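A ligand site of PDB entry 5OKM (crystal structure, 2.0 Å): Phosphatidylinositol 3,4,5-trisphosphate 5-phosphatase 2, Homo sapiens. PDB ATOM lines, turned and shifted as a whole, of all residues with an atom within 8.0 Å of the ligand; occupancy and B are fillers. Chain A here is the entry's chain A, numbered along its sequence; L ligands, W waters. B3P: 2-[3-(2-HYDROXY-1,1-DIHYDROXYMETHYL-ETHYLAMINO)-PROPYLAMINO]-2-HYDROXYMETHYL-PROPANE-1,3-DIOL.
Water W4 lies within hydrogen-bond range of an oxygen (O2) of the ligand, the backbone carbonyl oxygen (O) of Thr 37, the backbone NH (N) of Glu 40 and the backbone NH (N) of Asp 39.
Water W2 bridges O1 of the ligand and O of Gly 35.
Water W1 bridges the backbone carbonyl oxygen (O) of Gly 35 and a nitrogen (N2) of the ligand.
Water W3 bridges an oxygen (O4) of the ligand (3.1 Å) and the side-chain carboxylate (OD1) of Asp 294 (3.2 Å).
The side-chain hydroxyl (OG1) of Thr 37 lies within hydrogen-bond range of a nitrogen (N2) of the ligand, 2.8 Å away.
An oxygen (O2) of the ligand sits close to the backbone NH (N) of Asp 39 (3.5 Å).
OD2 of Asp 294 is in hydrogen-bond range of O5 of the ligand (2.8 Å).
The backbone carbonyl oxygen of Gly 33 sits at hydrogen-bond distance from a nitrogen (N1) of the ligand, 2.7 Å away.
OD1 of Asp 39 is in hydrogen-bond range of O4 of the ligand (2.6 Å).
Residues that only touch the ligand: Glu 40 (3.5 Å), Gly 35 (3.6 Å) and Leu 34 (3.8 Å).
Hydrophobic or aromatic side chains within 4 Å of the ligand: Leu 34.
Of the 22 residues printed, 7 come within 4 Å of the ligand.
Along chain A the residues within 4 Å of the ligand span positions 33 to 294.
The side-chain hydroxyl (OG1) of Thr 37 is in hydrogen-bond range of the side-chain carboxylate (OD2) of Asp 39.
OD2 of Asp 39 sits at hydrogen-bond distance from N of Gly 33, at 3.0 Å.
N of Leu 34 lies within hydrogen-bond range of O of Cys 292, 2.7 Å away.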
ATOM      1  N   SER A  27       8.742  37.933 -20.593  1.00  0.00           N
ATOM      2  CA  SER A  27       9.223  36.771 -19.857  1.00  0.00           C
ATOM      3  C   SER A  27       8.996  36.870 -18.346  1.00  0.00           C
ATOM      4  O   SER A  27       8.678  35.878 -17.700  1.00  0.00           O
ATOM      5  CB  SER A  27      10.711  36.574 -20.125  1.00  0.00           C
ATOM      6  OG  SER A  27      10.904  36.118 -21.455  1.00  0.00           O
ATOM      7  N   SER A  31       6.314  34.277 -16.335  1.00  0.00           N
ATOM      8  CA  SER A  31       7.081  33.264 -15.582  1.00  0.00           C
ATOM      9  C   SER A  31       7.923  32.348 -16.490  1.00  0.00           C
ATOM     10  O   SER A  31       7.907  31.101 -16.325  1.00  0.00           O
ATOM     11  CB  SER A  31       6.180  32.432 -14.679  1.00  0.00           C
ATOM     12  OG  SER A  31       5.522  33.200 -13.713  1.00  0.00           O
ATOM     13  N   LYS A  32       8.627  32.952 -17.450  1.00  0.00           N
ATOM     14  CA  LYS A  32       9.484  32.203 -18.360  1.00  0.00           C
ATOM     15  C   LYS A  32      10.929  32.457 -18.002  1.00  0.00           C
ATOM     16  O   LYS A  32      11.335  33.588 -17.760  1.00  0.00           O
ATOM     17  CB  LYS A  32       9.217  32.588 -19.814  1.00  0.00           C
ATOM     18  CG  LYS A  32       7.855  32.122 -20.313  1.00  0.00           C
ATOM     19  CD  LYS A  32       7.684  32.374 -21.814  1.00  0.00           C
ATOM     20  CE  LYS A  32       6.283  31.988 -22.279  1.00  0.00           C
ATOM     21  NZ  LYS A  32       6.128  32.144 -23.756  1.00  0.00           N
ATOM     22  N   GLY A  33      11.709  31.380 -17.940  1.00  0.00           N
ATOM     23  CA  GLY A  33      13.145  31.510 -17.717  1.00  0.00           C
ATOM     24  C   GLY A  33      13.707  30.310 -16.987  1.00  0.00           C
ATOM     25  O   GLY A  33      13.677  29.193 -17.521  1.00  0.00           O
ATOM     26  N   LEU A  34      14.207  30.529 -15.772  1.00  0.00           N
ATOM     27  CA  LEU A  34      14.881  29.491 -15.011  1.00  0.00           C
ATOM     28  C   LEU A  34      14.160  29.248 -13.704  1.00  0.00           C
ATOM     29  O   LEU A  34      13.554  30.158 -13.122  1.00  0.00           O
ATOM     30  CB  LEU A  34      16.336  29.893 -14.757  1.00  0.00           C
ATOM     31  CG  LEU A  34      17.194  30.202 -16.012  1.00  0.00           C
ATOM     32  CD1 LEU A  34      18.580  30.749 -15.636  1.00  0.00           C
ATOM     33  CD2 LEU A  34      17.360  28.958 -16.886  1.00  0.00           C
ATOM     34  N   GLY A  35      14.240  28.003 -13.231  1.00  0.00           N
ATOM     35  CA  GLY A  35      13.662  27.593 -11.956  1.00  0.00           C
ATOM     36  C   GLY A  35      12.382  26.790 -12.123  1.00  0.00           C
ATOM     37  O   GLY A  35      12.310  25.867 -12.948  1.00  0.00           O
ATOM     38  N   LYS A  36      11.378  27.109 -11.291  1.00  0.00           N
ATOM     39  CA  LYS A  36      10.035  26.565 -11.418  1.00  0.00           C
ATOM     40  C   LYS A  36       9.210  27.554 -12.276  1.00  0.00           C
ATOM     41  O   LYS A  36       8.811  28.620 -11.816  1.00  0.00           O
ATOM     42  CB  LYS A  36       9.409  26.344 -10.052  1.00  0.00           C
ATOM     43  CG  LYS A  36       8.064  25.663 -10.146  1.00  0.00           C
ATOM     44  CD  LYS A  36       7.438  25.443  -8.781  1.00  0.00           C
ATOM     45  CE  LYS A  36       6.373  24.361  -8.881  1.00  0.00           C
ATOM     46  NZ  LYS A  36       5.305  24.629  -7.922  1.00  0.00           N
ATOM     47  N   THR A  37       9.000  27.188 -13.525  1.00  0.00           N
ATOM     48  CA  THR A  37       8.532  28.134 -14.542  1.00  0.00           C
ATOM     49  C   THR A  37       7.258  27.665 -15.214  1.00  0.00           C
ATOM     50  O   THR A  37       6.885  26.482 -15.142  1.00  0.00           O
ATOM     51  CB  THR A  37       9.588  28.417 -15.648  1.00  0.00           C
ATOM     52  OG1 THR A  37       9.596  27.339 -16.596  1.00  0.00           O
ATOM     53  CG2 THR A  37      10.969  28.605 -15.069  1.00  0.00           C
ATOM     54  N   LEU A  38       6.633  28.598 -15.916  1.00  0.00           N
ATOM     55  CA  LEU A  38       5.452  28.322 -16.738  1.00  0.00           C
ATOM     56  C   LEU A  38       5.822  28.286 -18.208  1.00  0.00           C
ATOM     57  O   LEU A  38       4.990  28.600 -19.052  1.00  0.00           O
ATOM     58  CB  LEU A  38       4.370  29.389 -16.478  1.00  0.00           C
ATOM     59  CG  LEU A  38       3.901  29.486 -15.025  1.00  0.00           C
ATOM     60  CD1 LEU A  38       2.832  30.584 -14.912  1.00  0.00           C
ATOM     61  CD2 LEU A  38       3.384  28.134 -14.494  1.00  0.00           C
ATOM     62  N   ASP A  39       7.064  27.901 -18.529  1.00  0.00           N
ATOM     63  CA  ASP A  39       7.523  27.831 -19.920  1.00  0.00           C
ATOM     64  C   ASP A  39       6.732  26.834 -20.798  1.00  0.00           C
ATOM     65  O   ASP A  39       6.622  27.042 -21.998  1.00  0.00           O
ATOM     66  CB  ASP A  39       9.020  27.472 -19.996  1.00  0.00           C
ATOM     67  CG  ASP A  39       9.923  28.665 -19.762  1.00  0.00           C
ATOM     68  OD1 ASP A  39      10.082  29.480 -20.695  1.00  0.00           O
ATOM     69  OD2 ASP A  39      10.499  28.785 -18.655  1.00  0.00           O
ATOM     70  N   GLU A  40       6.199  25.775 -20.188  1.00  0.00           N
ATOM     71  CA  GLU A  40       5.358  24.790 -20.908  1.00  0.00           C
ATOM     72  C   GLU A  40       4.039  25.371 -21.440  1.00  0.00           C
ATOM     73  O   GLU A  40       3.510  24.879 -22.437  1.00  0.00           O
ATOM     74  CB  GLU A  40       5.061  23.554 -20.026  1.00  0.00           C
ATOM     75  CG  GLU A  40       4.094  23.805 -18.865  1.00  0.00           C
ATOM     76  CD  GLU A  40       3.888  22.590 -17.968  1.00  0.00           C
ATOM     77  OE1 GLU A  40       3.770  22.774 -16.733  1.00  0.00           O
ATOM     78  OE2 GLU A  40       3.832  21.436 -18.482  1.00  0.00           O
ATOM     79  N   VAL A  41       3.520  26.415 -20.776  1.00  0.00           N
ATOM     80  CA  VAL A  41       2.249  27.048 -21.176  1.00  0.00           C
ATOM     81  C   VAL A  41       2.377  27.791 -22.528  1.00  0.00           C
ATOM     82  O   VAL A  41       3.173  28.722 -22.672  1.00  0.00           O
ATOM     83  CB  VAL A  41       1.724  28.059 -20.123  1.00  0.00           C
ATOM     84  CG1 VAL A  41       0.388  28.657 -20.555  1.00  0.00           C
ATOM     85  CG2 VAL A  41       1.562  27.402 -18.752  1.00  0.00           C
ATOM     86  N   LYS A 209      25.276  23.807 -12.171  1.00  0.00           N
ATOM     87  CA  LYS A 209      23.874  23.841 -11.728  1.00  0.00           C
ATOM     88  C   LYS A 209      23.615  23.010 -10.468  1.00  0.00           C
ATOM     89  O   LYS A 209      22.605  22.317 -10.356  1.00  0.00           O
ATOM     90  CB  LYS A 209      22.939  23.448 -12.866  1.00  0.00           C
ATOM     91  CG  LYS A 209      22.971  24.457 -14.035  1.00  0.00           C
ATOM     92  CD  LYS A 209      22.255  23.959 -15.296  1.00  0.00           C
ATOM     93  CE  LYS A 209      21.045  23.073 -14.975  1.00  0.00           C
ATOM     94  NZ  LYS A 209      20.249  22.723 -16.176  1.00  0.00           N
ATOM     95  N   SER A 239      15.331  26.647  -7.581  1.00  0.00           N
ATOM     96  CA  SER A 239      16.045  25.869  -8.598  1.00  0.00           C
ATOM     97  C   SER A 239      16.540  26.773  -9.733  1.00  0.00           C
ATOM     98  O   SER A 239      16.747  26.320 -10.837  1.00  0.00           O
ATOM     99  CB  SER A 239      15.127  24.755  -9.128  1.00  0.00           C
ATOM    100  OG  SER A 239      13.999  25.343  -9.753  1.00  0.00           O
ATOM    101  N   ASN A 288       2.540  28.000  -8.032  1.00  0.00           N
ATOM    102  CA  ASN A 288       2.670  27.430  -9.382  1.00  0.00           C
ATOM    103  C   ASN A 288       3.955  27.838 -10.144  1.00  0.00           C
ATOM    104  O   ASN A 288       4.299  27.207 -11.141  1.00  0.00           O
ATOM    105  CB  ASN A 288       1.430  27.792 -10.217  1.00  0.00           C
ATOM    106  CG  ASN A 288       0.167  27.067  -9.762  1.00  0.00           C
ATOM    107  OD1 ASN A 288      -0.910  27.680  -9.627  1.00  0.00           O
ATOM    108  ND2 ASN A 288       0.292  25.778  -9.523  1.00  0.00           N
ATOM    109  N   SER A 289       4.650  28.870  -9.697  1.00  0.00           N
ATOM    110  CA  SER A 289       5.968  29.191 -10.265  1.00  0.00           C
ATOM    111  C   SER A 289       6.807  30.000  -9.290  1.00  0.00           C
ATOM    112  O   SER A 289       6.277  30.711  -8.440  1.00  0.00           O
ATOM    113  CB  SER A 289       5.817  29.951 -11.602  1.00  0.00           C
ATOM    114  OG  SER A 289       5.347  31.283 -11.433  1.00  0.00           O
ATOM    115  N   TYR A 290       8.116  29.845  -9.408  1.00  0.00           N
ATOM    116  CA  TYR A 290       9.102  30.603  -8.646  1.00  0.00           C
ATOM    117  C   TYR A 290      10.398  30.475  -9.388  1.00  0.00           C
ATOM    118  O   TYR A 290      11.010  29.385  -9.473  1.00  0.00           O
ATOM    119  CB  TYR A 290       9.251  30.119  -7.219  1.00  0.00           C
ATOM    120  CG  TYR A 290      10.120  30.982  -6.316  1.00  0.00           C
ATOM    121  CD1 TYR A 290      10.047  32.375  -6.351  1.00  0.00           C
ATOM    122  CD2 TYR A 290      10.970  30.398  -5.361  1.00  0.00           C
ATOM    123  CE1 TYR A 290      10.812  33.155  -5.496  1.00  0.00           C
ATOM    124  CE2 TYR A 290      11.730  31.172  -4.491  1.00  0.00           C
ATOM    125  CZ  TYR A 290      11.637  32.557  -4.583  1.00  0.00           C
ATOM    126  OH  TYR A 290      12.369  33.364  -3.735  1.00  0.00           O
ATOM    127  N   CYS A 292      13.479  32.953 -12.102  1.00  0.00           N
ATOM    128  CA  CYS A 292      14.015  34.193 -12.627  1.00  0.00           C
ATOM    129  C   CYS A 292      14.039  34.150 -14.149  1.00  0.00           C
ATOM    130  O   CYS A 292      14.068  33.067 -14.760  1.00  0.00           O
ATOM    131  CB  CYS A 292      15.422  34.460 -12.071  1.00  0.00           C
ATOM    132  SG  CYS A 292      16.710  33.359 -12.714  1.00  0.00           S
ATOM    133  N   THR A 293      13.981  35.334 -14.766  1.00  0.00           N
ATOM    134  CA  THR A 293      14.169  35.434 -16.192  1.00  0.00           C
ATOM    135  C   THR A 293      15.651  35.333 -16.488  1.00  0.00           C
ATOM    136  O   THR A 293      16.489  35.499 -15.609  1.00  0.00           O
ATOM    137  CB  THR A 293      13.656  36.778 -16.764  1.00  0.00           C
ATOM    138  OG1 THR A 293      14.347  37.866 -16.123  1.00  0.00           O
ATOM    139  CG2 THR A 293      12.170  36.908 -16.543  1.00  0.00           C
ATOM    140  N   ASP A 294      15.960  35.032 -17.743  1.00  0.00           N
ATOM    141  CA  ASP A 294      17.340  35.079 -18.226  1.00  0.00           C
ATOM    142  C   ASP A 294      17.517  35.888 -19.506  1.00  0.00           C
ATOM    143  O   ASP A 294      18.590  35.908 -20.048  1.00  0.00           O
ATOM    144  CB  ASP A 294      17.934  33.650 -18.364  1.00  0.00           C
ATOM    145  CG  ASP A 294      17.325  32.851 -19.502  1.00  0.00           C
ATOM    146  OD1 ASP A 294      16.462  33.370 -20.210  1.00  0.00           O
ATOM    147  OD2 ASP A 294      17.718  31.674 -19.692  1.00  0.00           O
ATOM    148  N   ASP A 295      16.462  36.552 -19.959  1.00  0.00           N
ATOM    149  CA  ASP A 295      16.544  37.383 -21.179  1.00  0.00           C
ATOM    150  C   ASP A 295      16.394  38.882 -20.866  1.00  0.00           C
ATOM    151  O   ASP A 295      16.304  39.694 -21.786  1.00  0.00           O
ATOM    152  CB  ASP A 295      15.514  36.928 -22.219  1.00  0.00           C
ATOM    153  CG  ASP A 295      14.070  36.997 -21.717  1.00  0.00           C
ATOM    154  OD1 ASP A 295      13.839  37.401 -20.555  1.00  0.00           O
ATOM    155  OD2 ASP A 295      13.152  36.642 -22.474  1.00  0.00           O
ATOM    156  N   PHE A 305      10.127  36.006 -10.508  1.00  0.00           N
ATOM    157  CA  PHE A 305       8.679  35.834 -10.549  1.00  0.00           C
ATOM    158  C   PHE A 305       8.200  34.762  -9.566  1.00  0.00           C
ATOM    159  O   PHE A 305       8.913  33.828  -9.282  1.00  0.00           O
ATOM    160  CB  PHE A 305       8.156  35.541 -11.975  1.00  0.00           C
ATOM    161  CG  PHE A 305       8.938  34.485 -12.707  1.00  0.00           C
ATOM    162  CD1 PHE A 305       8.728  33.136 -12.452  1.00  0.00           C
ATOM    163  CD2 PHE A 305       9.883  34.838 -13.652  1.00  0.00           C
ATOM    164  CE1 PHE A 305       9.459  32.156 -13.124  1.00  0.00           C
ATOM    165  CE2 PHE A 305      10.606  33.871 -14.347  1.00  0.00           C
ATOM    166  CZ  PHE A 305      10.402  32.538 -14.077  1.00  0.00           C
HETATM  167  C1  B3P L   1      12.921  26.393 -18.222  1.00  0.00           C
HETATM  168  C2  B3P L   1      11.926  25.245 -18.205  1.00  0.00           C
HETATM  169  C3  B3P L   1      13.453  26.570 -19.640  1.00  0.00           C
HETATM  170  N1  B3P L   1      14.245  27.830 -19.763  1.00  0.00           N
HETATM  171  C4  B3P L   1      14.558  28.228 -21.162  1.00  0.00           C
HETATM  172  C5  B3P L   1      13.263  28.669 -21.858  1.00  0.00           C
HETATM  173  C6  B3P L   1      15.477  29.471 -21.226  1.00  0.00           C
HETATM  174  C7  B3P L   1      15.203  27.064 -21.944  1.00  0.00           C
HETATM  175  N2  B3P L   1      11.375  25.184 -16.850  1.00  0.00           N
HETATM  176  C8  B3P L   1      10.542  24.004 -16.515  1.00  0.00           C
HETATM  177  C9  B3P L   1       9.922  24.366 -15.158  1.00  0.00           C
HETATM  178  C10 B3P L   1       9.432  23.720 -17.559  1.00  0.00           C
HETATM  179  C11 B3P L   1      11.423  22.744 -16.388  1.00  0.00           C
HETATM  180  O1  B3P L   1       9.115  23.363 -14.579  1.00  0.00           O
HETATM  181  O2  B3P L   1       8.643  24.869 -17.839  1.00  0.00           O
HETATM  182  O3  B3P L   1      10.618  21.596 -16.129  1.00  0.00           O
HETATM  183  O4  B3P L   1      12.613  29.642 -21.014  1.00  0.00           O
HETATM  184  O5  B3P L   1      16.747  29.242 -20.620  1.00  0.00           O
HETATM  185  O6  B3P L   1      16.255  26.413 -21.195  1.00  0.00           O
HETATM  186  O   HOH W   1      13.553  24.724 -14.912  1.00  0.00           O
HETATM  187  O   HOH W   2      11.240  22.678 -12.651  1.00  0.00           O
HETATM  188  O   HOH W   3      13.650  32.532 -21.471  1.00  0.00           O
HETATM  189  O   HOH W   4       6.316  24.881 -17.038  1.00  0.00           O
